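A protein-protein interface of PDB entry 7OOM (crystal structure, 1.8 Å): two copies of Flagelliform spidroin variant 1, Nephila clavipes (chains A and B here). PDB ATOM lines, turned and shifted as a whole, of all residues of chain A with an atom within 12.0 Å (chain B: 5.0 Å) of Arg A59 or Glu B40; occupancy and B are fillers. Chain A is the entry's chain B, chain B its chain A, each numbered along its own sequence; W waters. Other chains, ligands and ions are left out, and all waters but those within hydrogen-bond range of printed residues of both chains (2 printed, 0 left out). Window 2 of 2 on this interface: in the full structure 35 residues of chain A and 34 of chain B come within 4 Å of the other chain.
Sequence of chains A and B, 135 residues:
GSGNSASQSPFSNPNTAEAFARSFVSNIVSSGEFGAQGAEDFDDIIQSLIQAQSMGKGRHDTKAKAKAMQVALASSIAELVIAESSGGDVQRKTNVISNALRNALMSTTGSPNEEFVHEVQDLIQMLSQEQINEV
The side-chain carboxylate (OE2) of Glu B40 lies within salt-bridge range of the guanidinium group (NH2) of Arg A59. OD2 of Asp B44 lies within salt-bridge range of NZ of Lys A65, 2.6 Å away. OD1 of Asp B41 sits at hydrogen-bond distance from OG1 of Thr A62 (3.2 Å).
The side-chain carboxylate (OD1) of Asp B41 sits at hydrogen-bond distance from the side-chain amide nitrogen (NE2) of Gln B37 (3.3 Å). O of Lys A57 is in hydrogen-bond range of NZ of Lys A65, at 2.8 Å. The backbone NH of Lys A65 is in hydrogen-bond range of the side-chain hydroxyl of Thr A62 (3.3 Å). O of His A60 lies within hydrogen-bond range of NZ of Lys A65. The backbone carbonyl oxygen (O) of Gly A56 lies within hydrogen-bond range of the side-chain amino group (NZ) of Lys A65, at 3.0 Å.
Gly A56 touches Asp B44. OD2 of Asp B44 touches CA of Gly A58, 3.9 Å away. Gln B37 touches Thr A62. Lys A65 touches Asp B41. CD1 of Ile B45 touches O of Lys A65, 3.7 Å away. CG of Met A69 touches CD1 of Ile B45 (3.5 Å).
Printed residues of chain B within 4 Å of Arg A59: Glu B40 (2.6 Å). Glu B40 touches just one residue of chain A: Arg A59. Gln B37 touches one residue of chain A. No residue of chain A comes within 4 Å of Gly B38. No residue of chain A comes within 4 Å of Ala B39. Of chain A, only Thr A62 and Lys A65 come within 4 Å of Asp B41. No residue of chain A comes within 4 Å of Asp B43. Asp B44 touches just these residues of chain A: Gly A56, Gly A58 and Lys A65. Printed residues of chain B within 4 Å of Met A69: Ile B45. Of the printed residues of chain B, Thr A62 touches Gln B37 and Asp B41. Printed residues of chain B within 4 Å of Gly A56: Asp B44 (3.7 Å). Printed residues of chain A within 4 Å of Ile B45: Lys A65 and Met A69. Gln A51 touches none of the printed residues of chain B.
Printed residues of chain A that touch a printed residue of chain B: Gly A56, Gly A58, Arg A59, Thr A62, Lys A65 and Met A69. Of the 10 printed residues of chain B, 5 touch a printed residue of chain A. Hydrophobic or aromatic side chains of chain B within 4 Å of the printed part of chain A: Ile B45. Along chain B the printed residues that touch a printed residue of chain A span positions 37 to 45. Among the printed residues, 9 pairs touch across the chains. Among the printed residues, Asp or Glu carboxylates within 4 Å of a Lys or Arg side-chain nitrogen of the other chain: Arg A59 with Glu B40 (2.6 Å) and Lys A65 with Asp B44 (2.6 Å).
No position is printed for both chains.
Water W2 bridges the side-chain carboxylate of Asp B41 (2.6 Å) and the side-chain hydroxyl of Thr A62 (3.1 Å). Water W1 lies within hydrogen-bond range of OD1 of Asp B44, OE2 of Glu B40 and N of Arg A59.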
ATOM      1  N   GLN A  51     -28.953  -0.491 -11.843  1.00  0.00           N
ATOM      2  CA  GLN A  51     -27.857  -1.392 -12.247  1.00  0.00           C
ATOM      3  C   GLN A  51     -27.238  -0.858 -13.539  1.00  0.00           C
ATOM      4  O   GLN A  51     -25.998  -0.843 -13.665  1.00  0.00           O
ATOM      5  CB  GLN A  51     -28.382  -2.805 -12.450  1.00  0.00           C
ATOM      6  CG  GLN A  51     -29.022  -3.377 -11.191  1.00  0.00           C
ATOM      7  CD  GLN A  51     -29.185  -4.870 -11.295  1.00  0.00           C
ATOM      8  OE1 GLN A  51     -29.091  -5.589 -10.309  1.00  0.00           O
ATOM      9  NE2 GLN A  51     -29.393  -5.357 -12.506  1.00  0.00           N
ATOM     10  N   ALA A  52     -28.073  -0.435 -14.483  1.00  0.00           N
ATOM     11  CA  ALA A  52     -27.603   0.101 -15.778  1.00  0.00           C
ATOM     12  C   ALA A  52     -26.746   1.360 -15.565  1.00  0.00           C
ATOM     13  O   ALA A  52     -25.718   1.479 -16.283  1.00  0.00           O
ATOM     14  CB  ALA A  52     -28.783   0.377 -16.674  1.00  0.00           C
ATOM     15  N   GLN A  53     -27.160   2.249 -14.669  1.00  0.00           N
ATOM     16  CA  GLN A  53     -26.481   3.531 -14.332  1.00  0.00           C
ATOM     17  C   GLN A  53     -25.060   3.234 -13.836  1.00  0.00           C
ATOM     18  O   GLN A  53     -24.091   3.912 -14.252  1.00  0.00           O
ATOM     19  CB  GLN A  53     -27.270   4.290 -13.272  1.00  0.00           C
ATOM     20  CG  GLN A  53     -26.769   5.706 -13.009  1.00  0.00           C
ATOM     21  CD  GLN A  53     -27.528   6.795 -13.743  1.00  0.00           C
ATOM     22  OE1 GLN A  53     -26.944   7.804 -14.153  1.00  0.00           O
ATOM     23  NE2 GLN A  53     -28.840   6.623 -13.897  1.00  0.00           N
ATOM     24  N   SER A  54     -24.916   2.218 -12.998  1.00  0.00           N
ATOM     25  CA  SER A  54     -23.578   1.793 -12.497  1.00  0.00           C
ATOM     26  C   SER A  54     -22.749   1.206 -13.631  1.00  0.00           C
ATOM     27  O   SER A  54     -21.612   1.664 -13.820  1.00  0.00           O
ATOM     28  CB  SER A  54     -23.688   0.827 -11.352  1.00  0.00           C
ATOM     29  OG  SER A  54     -22.429   0.693 -10.727  1.00  0.00           O
ATOM     30  N   MET A  55     -23.287   0.216 -14.348  1.00  0.00           N
ATOM     31  CA  MET A  55     -22.623  -0.481 -15.486  1.00  0.00           C
ATOM     32  C   MET A  55     -22.255   0.543 -16.563  1.00  0.00           C
ATOM     33  O   MET A  55     -21.167   0.431 -17.139  1.00  0.00           O
ATOM     34  CB  MET A  55     -23.542  -1.541 -16.105  1.00  0.00           C
ATOM     35  CG  MET A  55     -22.903  -2.284 -17.261  1.00  0.00           C
ATOM     36  SD  MET A  55     -23.487  -3.984 -17.423  1.00  0.00           S
ATOM     37  CE  MET A  55     -22.775  -4.437 -18.999  1.00  0.00           C
ATOM     38  N   GLY A  56     -23.113   1.536 -16.783  1.00  0.00           N
ATOM     39  CA  GLY A  56     -22.907   2.540 -17.848  1.00  0.00           C
ATOM     40  C   GLY A  56     -21.643   3.366 -17.621  1.00  0.00           C
ATOM     41  O   GLY A  56     -21.140   3.945 -18.603  1.00  0.00           O
ATOM     42  N   LYS A  57     -21.119   3.413 -16.389  1.00  0.00           N
ATOM     43  CA  LYS A  57     -19.842   4.126 -16.087  1.00  0.00           C
ATOM     44  C   LYS A  57     -18.670   3.520 -16.893  1.00  0.00           C
ATOM     45  O   LYS A  57     -17.766   4.277 -17.306  1.00  0.00           O
ATOM     46  CB  LYS A  57     -19.644   4.167 -14.565  1.00  0.00           C
ATOM     47  CG  LYS A  57     -20.673   5.035 -13.850  1.00  0.00           C
ATOM     48  CD  LYS A  57     -20.444   5.298 -12.370  1.00  0.00           C
ATOM     49  CE  LYS A  57     -21.529   6.210 -11.827  1.00  0.00           C
ATOM     50  NZ  LYS A  57     -21.247   6.641 -10.443  1.00  0.00           N
ATOM     51  N   GLY A  58     -18.715   2.224 -17.185  1.00  0.00           N
ATOM     52  CA  GLY A  58     -17.638   1.445 -17.804  1.00  0.00           C
ATOM     53  C   GLY A  58     -16.284   1.877 -17.263  1.00  0.00           C
ATOM     54  O   GLY A  58     -16.179   2.133 -16.040  1.00  0.00           O
ATOM     55  N   ARG A  59     -15.311   1.971 -18.164  1.00  0.00           N
ATOM     56  CA  ARG A  59     -13.871   2.151 -17.863  1.00  0.00           C
ATOM     57  C   ARG A  59     -13.611   3.548 -17.289  1.00  0.00           C
ATOM     58  O   ARG A  59     -12.668   3.706 -16.494  1.00  0.00           O
ATOM     59  CB  ARG A  59     -13.083   1.946 -19.160  1.00  0.00           C
ATOM     60  CG  ARG A  59     -11.691   1.386 -18.933  1.00  0.00           C
ATOM     61  CD  ARG A  59     -10.604   2.279 -19.495  1.00  0.00           C
ATOM     62  NE  ARG A  59     -10.845   2.746 -20.850  1.00  0.00           N
ATOM     63  CZ  ARG A  59     -11.130   1.975 -21.891  1.00  0.00           C
ATOM     64  NH1 ARG A  59     -11.273   0.664 -21.764  1.00  0.00           N
ATOM     65  NH2 ARG A  59     -11.276   2.535 -23.079  1.00  0.00           N
ATOM     66  N   HIS A  60     -14.374   4.547 -17.743  1.00  0.00           N
ATOM     67  CA  HIS A  60     -14.234   5.975 -17.375  1.00  0.00           C
ATOM     68  C   HIS A  60     -15.621   6.627 -17.499  1.00  0.00           C
ATOM     69  O   HIS A  60     -16.187   6.474 -18.571  1.00  0.00           O
ATOM     70  CB  HIS A  60     -13.199   6.653 -18.299  1.00  0.00           C
ATOM     71  CG  HIS A  60     -12.844   8.020 -17.832  1.00  0.00           C
ATOM     72  ND1 HIS A  60     -13.473   9.153 -18.321  1.00  0.00           N
ATOM     73  CD2 HIS A  60     -11.987   8.434 -16.871  1.00  0.00           C
ATOM     74  CE1 HIS A  60     -12.998  10.211 -17.694  1.00  0.00           C
ATOM     75  NE2 HIS A  60     -12.078   9.799 -16.798  1.00  0.00           N
ATOM     76  N   ASP A  61     -16.153   7.199 -16.420  1.00  0.00           N
ATOM     77  CA  ASP A  61     -17.451   7.926 -16.433  1.00  0.00           C
ATOM     78  C   ASP A  61     -17.254   9.238 -17.195  1.00  0.00           C
ATOM     79  O   ASP A  61     -16.139   9.793 -17.190  1.00  0.00           O
ATOM     80  CB  ASP A  61     -18.027   8.206 -15.064  1.00  0.00           C
ATOM     81  CG  ASP A  61     -19.530   8.462 -15.119  1.00  0.00           C
ATOM     82  OD1 ASP A  61     -20.159   8.185 -16.177  1.00  0.00           O
ATOM     83  OD2 ASP A  61     -20.049   8.927 -14.125  1.00  0.00           O
ATOM     84  N   THR A  62     -18.243   9.619 -17.990  1.00  0.00           N
ATOM     85  CA  THR A  62     -18.194  10.864 -18.801  1.00  0.00           C
ATOM     86  C   THR A  62     -19.531  11.590 -18.605  1.00  0.00           C
ATOM     87  O   THR A  62     -20.534  10.927 -18.254  1.00  0.00           O
ATOM     88  CB  THR A  62     -17.896  10.598 -20.274  1.00  0.00           C
ATOM     89  OG1 THR A  62     -18.967   9.930 -20.933  1.00  0.00           O
ATOM     90  CG2 THR A  62     -16.665   9.753 -20.536  1.00  0.00           C
ATOM     91  N   LYS A  63     -19.529  12.899 -18.819  1.00  0.00           N
ATOM     92  CA  LYS A  63     -20.741  13.740 -18.669  1.00  0.00           C
ATOM     93  C   LYS A  63     -21.790  13.290 -19.694  1.00  0.00           C
ATOM     94  O   LYS A  63     -23.003  13.311 -19.358  1.00  0.00           O
ATOM     95  CB  LYS A  63     -20.343  15.207 -18.851  1.00  0.00           C
ATOM     96  CG  LYS A  63     -19.453  15.776 -17.747  1.00  0.00           C
ATOM     97  CD  LYS A  63     -20.173  15.986 -16.418  1.00  0.00           C
ATOM     98  CE  LYS A  63     -19.634  17.150 -15.607  1.00  0.00           C
ATOM     99  NZ  LYS A  63     -18.227  16.923 -15.201  1.00  0.00           N
ATOM    100  N   ALA A  64     -21.377  12.916 -20.902  1.00  0.00           N
ATOM    101  CA  ALA A  64     -22.324  12.518 -21.967  1.00  0.00           C
ATOM    102  C   ALA A  64     -22.991  11.219 -21.546  1.00  0.00           C
ATOM    103  O   ALA A  64     -24.237  11.091 -21.723  1.00  0.00           O
ATOM    104  CB  ALA A  64     -21.678  12.413 -23.324  1.00  0.00           C
ATOM    105  N   LYS A  65     -22.221  10.268 -20.972  1.00  0.00           N
ATOM    106  CA  LYS A  65     -22.841   8.995 -20.530  1.00  0.00           C
ATOM    107  C   LYS A  65     -23.803   9.228 -19.352  1.00  0.00           C
ATOM    108  O   LYS A  65     -24.866   8.593 -19.338  1.00  0.00           O
ATOM    109  CB  LYS A  65     -21.782   7.943 -20.268  1.00  0.00           C
ATOM    110  CG  LYS A  65     -21.237   7.306 -21.541  1.00  0.00           C
ATOM    111  CD  LYS A  65     -20.379   6.104 -21.218  1.00  0.00           C
ATOM    112  CE  LYS A  65     -19.296   6.408 -20.215  1.00  0.00           C
ATOM    113  NZ  LYS A  65     -18.657   5.135 -19.798  1.00  0.00           N
ATOM    114  N   ALA A  66     -23.475  10.087 -18.407  1.00  0.00           N
ATOM    115  CA  ALA A  66     -24.337  10.361 -17.247  1.00  0.00           C
ATOM    116  C   ALA A  66     -25.671  10.938 -17.769  1.00  0.00           C
ATOM    117  O   ALA A  66     -26.729  10.531 -17.260  1.00  0.00           O
ATOM    118  CB  ALA A  66     -23.618  11.253 -16.262  1.00  0.00           C
ATOM    119  N   ALA A  68     -27.048  10.492 -20.813  1.00  0.00           N
ATOM    120  CA  ALA A  68     -27.728   9.377 -21.524  1.00  0.00           C
ATOM    121  C   ALA A  68     -28.433   8.478 -20.515  1.00  0.00           C
ATOM    122  O   ALA A  68     -29.589   8.109 -20.767  1.00  0.00           O
ATOM    123  CB  ALA A  68     -26.726   8.590 -22.344  1.00  0.00           C
ATOM    124  N   MET A  69     -27.816   8.167 -19.365  1.00  0.00           N
ATOM    125  CA  MET A  69     -28.427   7.233 -18.385  1.00  0.00           C
ATOM    126  C   MET A  69     -29.548   7.925 -17.590  1.00  0.00           C
ATOM    127  O   MET A  69     -30.532   7.256 -17.258  1.00  0.00           O
ATOM    128  CB  MET A  69     -27.338   6.667 -17.461  1.00  0.00           C
ATOM    129  CG  MET A  69     -26.405   5.632 -18.147  1.00  0.00           C
ATOM    130  SD  MET A  69     -27.177   4.228 -19.009  1.00  0.00           S
ATOM    131  CE  MET A  69     -28.642   4.044 -18.044  1.00  0.00           C
ATOM    132  N   ALA B  36     -12.647   7.636 -30.635  1.00  0.00           N
ATOM    133  CA  ALA B  36     -12.444   6.565 -29.650  1.00  0.00           C
ATOM    134  C   ALA B  36     -13.483   6.717 -28.540  1.00  0.00           C
ATOM    135  O   ALA B  36     -14.193   5.767 -28.291  1.00  0.00           O
ATOM    136  CB  ALA B  36     -11.035   6.671 -29.119  1.00  0.00           C
ATOM    137  N   GLN B  37     -13.574   7.898 -27.934  1.00  0.00           N
ATOM    138  CA  GLN B  37     -14.348   8.071 -26.676  1.00  0.00           C
ATOM    139  C   GLN B  37     -15.840   8.023 -27.039  1.00  0.00           C
ATOM    140  O   GLN B  37     -16.593   7.442 -26.264  1.00  0.00           O
ATOM    141  CB  GLN B  37     -13.909   9.332 -25.925  1.00  0.00           C
ATOM    142  CG  GLN B  37     -14.516   9.455 -24.532  1.00  0.00           C
ATOM    143  CD  GLN B  37     -14.126   8.327 -23.607  1.00  0.00           C
ATOM    144  OE1 GLN B  37     -12.963   8.184 -23.229  1.00  0.00           O
ATOM    145  NE2 GLN B  37     -15.099   7.505 -23.231  1.00  0.00           N
ATOM    146  N   GLY B  38     -16.242   8.616 -28.166  1.00  0.00           N
ATOM    147  CA  GLY B  38     -17.627   8.585 -28.654  1.00  0.00           C
ATOM    148  C   GLY B  38     -18.111   7.170 -28.926  1.00  0.00           C
ATOM    149  O   GLY B  38     -19.208   6.802 -28.462  1.00  0.00           O
ATOM    150  N   ALA B  39     -17.329   6.349 -29.632  1.00  0.00           N
ATOM    151  CA  ALA B  39     -17.738   4.954 -29.919  1.00  0.00           C
ATOM    152  C   ALA B  39     -17.875   4.160 -28.605  1.00  0.00           C
ATOM    153  O   ALA B  39     -18.861   3.387 -28.474  1.00  0.00           O
ATOM    154  CB  ALA B  39     -16.761   4.298 -30.863  1.00  0.00           C
ATOM    155  N   GLU B  40     -16.931   4.354 -27.688  1.00  0.00           N
ATOM    156  CA  GLU B  40     -16.891   3.758 -26.332  1.00  0.00           C
ATOM    157  C   GLU B  40     -18.129   4.213 -25.545  1.00  0.00           C
ATOM    158  O   GLU B  40     -18.727   3.354 -24.876  1.00  0.00           O
ATOM    159  CB  GLU B  40     -15.581   4.145 -25.638  1.00  0.00           C
ATOM    160  CG  GLU B  40     -15.463   3.601 -24.213  1.00  0.00           C
ATOM    161  CD  GLU B  40     -14.040   3.463 -23.687  1.00  0.00           C
ATOM    162  OE1 GLU B  40     -13.138   4.129 -24.243  1.00  0.00           O
ATOM    163  OE2 GLU B  40     -13.841   2.701 -22.716  1.00  0.00           O
ATOM    164  N   ASP B  41     -18.518   5.493 -25.667  1.00  0.00           N
ATOM    165  CA  ASP B  41     -19.722   6.049 -24.981  1.00  0.00           C
ATOM    166  C   ASP B  41     -20.896   5.179 -25.451  1.00  0.00           C
ATOM    167  O   ASP B  41     -21.619   4.589 -24.597  1.00  0.00           O
ATOM    168  CB  ASP B  41     -19.908   7.558 -25.244  1.00  0.00           C
ATOM    169  CG  ASP B  41     -18.984   8.538 -24.518  1.00  0.00           C
ATOM    170  OD1 ASP B  41     -18.295   8.129 -23.552  1.00  0.00           O
ATOM    171  OD2 ASP B  41     -18.922   9.738 -24.962  1.00  0.00           O
ATOM    172  N   PHE B  42     -21.089   5.037 -26.769  1.00  0.00           N
ATOM    173  CA  PHE B  42     -22.226   4.246 -27.281  1.00  0.00           C
ATOM    174  C   PHE B  42     -22.101   2.835 -26.718  1.00  0.00           C
ATOM    175  O   PHE B  42     -23.119   2.243 -26.406  1.00  0.00           O
ATOM    176  CB  PHE B  42     -22.336   4.259 -28.808  1.00  0.00           C
ATOM    177  CG  PHE B  42     -22.953   5.519 -29.359  1.00  0.00           C
ATOM    178  CD1 PHE B  42     -24.334   5.691 -29.394  1.00  0.00           C
ATOM    179  CD2 PHE B  42     -22.144   6.534 -29.847  1.00  0.00           C
ATOM    180  CE1 PHE B  42     -24.894   6.864 -29.866  1.00  0.00           C
ATOM    181  CE2 PHE B  42     -22.712   7.690 -30.361  1.00  0.00           C
ATOM    182  CZ  PHE B  42     -24.077   7.856 -30.364  1.00  0.00           C
ATOM    183  N   ASP B  43     -20.898   2.257 -26.731  1.00  0.00           N
ATOM    184  CA  ASP B  43     -20.747   0.822 -26.389  1.00  0.00           C
ATOM    185  C   ASP B  43     -21.146   0.621 -24.927  1.00  0.00           C
ATOM    186  O   ASP B  43     -21.870  -0.355 -24.667  1.00  0.00           O
ATOM    187  CB  ASP B  43     -19.321   0.347 -26.656  1.00  0.00           C
ATOM    188  CG  ASP B  43     -19.130  -1.163 -26.588  1.00  0.00           C
ATOM    189  OD1 ASP B  43     -19.984  -1.915 -27.118  1.00  0.00           O
ATOM    190  OD2 ASP B  43     -18.119  -1.562 -25.996  1.00  0.00           O
ATOM    191  N   ASP B  44     -20.640   1.484 -24.037  1.00  0.00           N
ATOM    192  CA  ASP B  44     -20.849   1.361 -22.573  1.00  0.00           C
ATOM    193  C   ASP B  44     -22.370   1.453 -22.357  1.00  0.00           C
ATOM    194  O   ASP B  44     -22.965   0.696 -21.519  1.00  0.00           O
ATOM    195  CB  ASP B  44     -20.095   2.427 -21.777  1.00  0.00           C
ATOM    196  CG  ASP B  44     -18.580   2.248 -21.712  1.00  0.00           C
ATOM    197  OD1 ASP B  44     -18.140   1.173 -22.090  1.00  0.00           O
ATOM    198  OD2 ASP B  44     -17.867   3.195 -21.303  1.00  0.00           O
ATOM    199  N   ILE B  45     -23.020   2.365 -23.076  1.00  0.00           N
ATOM    200  CA  ILE B  45     -24.440   2.675 -22.748  1.00  0.00           C
ATOM    201  C   ILE B  45     -25.318   1.546 -23.288  1.00  0.00           C
ATOM    202  O   ILE B  45     -26.206   1.044 -22.577  1.00  0.00           O
ATOM    203  CB  ILE B  45     -24.842   4.050 -23.317  1.00  0.00           C
ATOM    204  CG1 ILE B  45     -24.134   5.190 -22.583  1.00  0.00           C
ATOM    205  CG2 ILE B  45     -26.337   4.174 -23.291  1.00  0.00           C
ATOM    206  CD1 ILE B  45     -24.557   5.405 -21.167  1.00  0.00           C
HETATM  207  O   HOH W   1     -15.554   1.074 -21.211  1.00  0.00           O
HETATM  208  O   HOH W   2     -17.731  11.461 -23.351  1.00  0.00           O
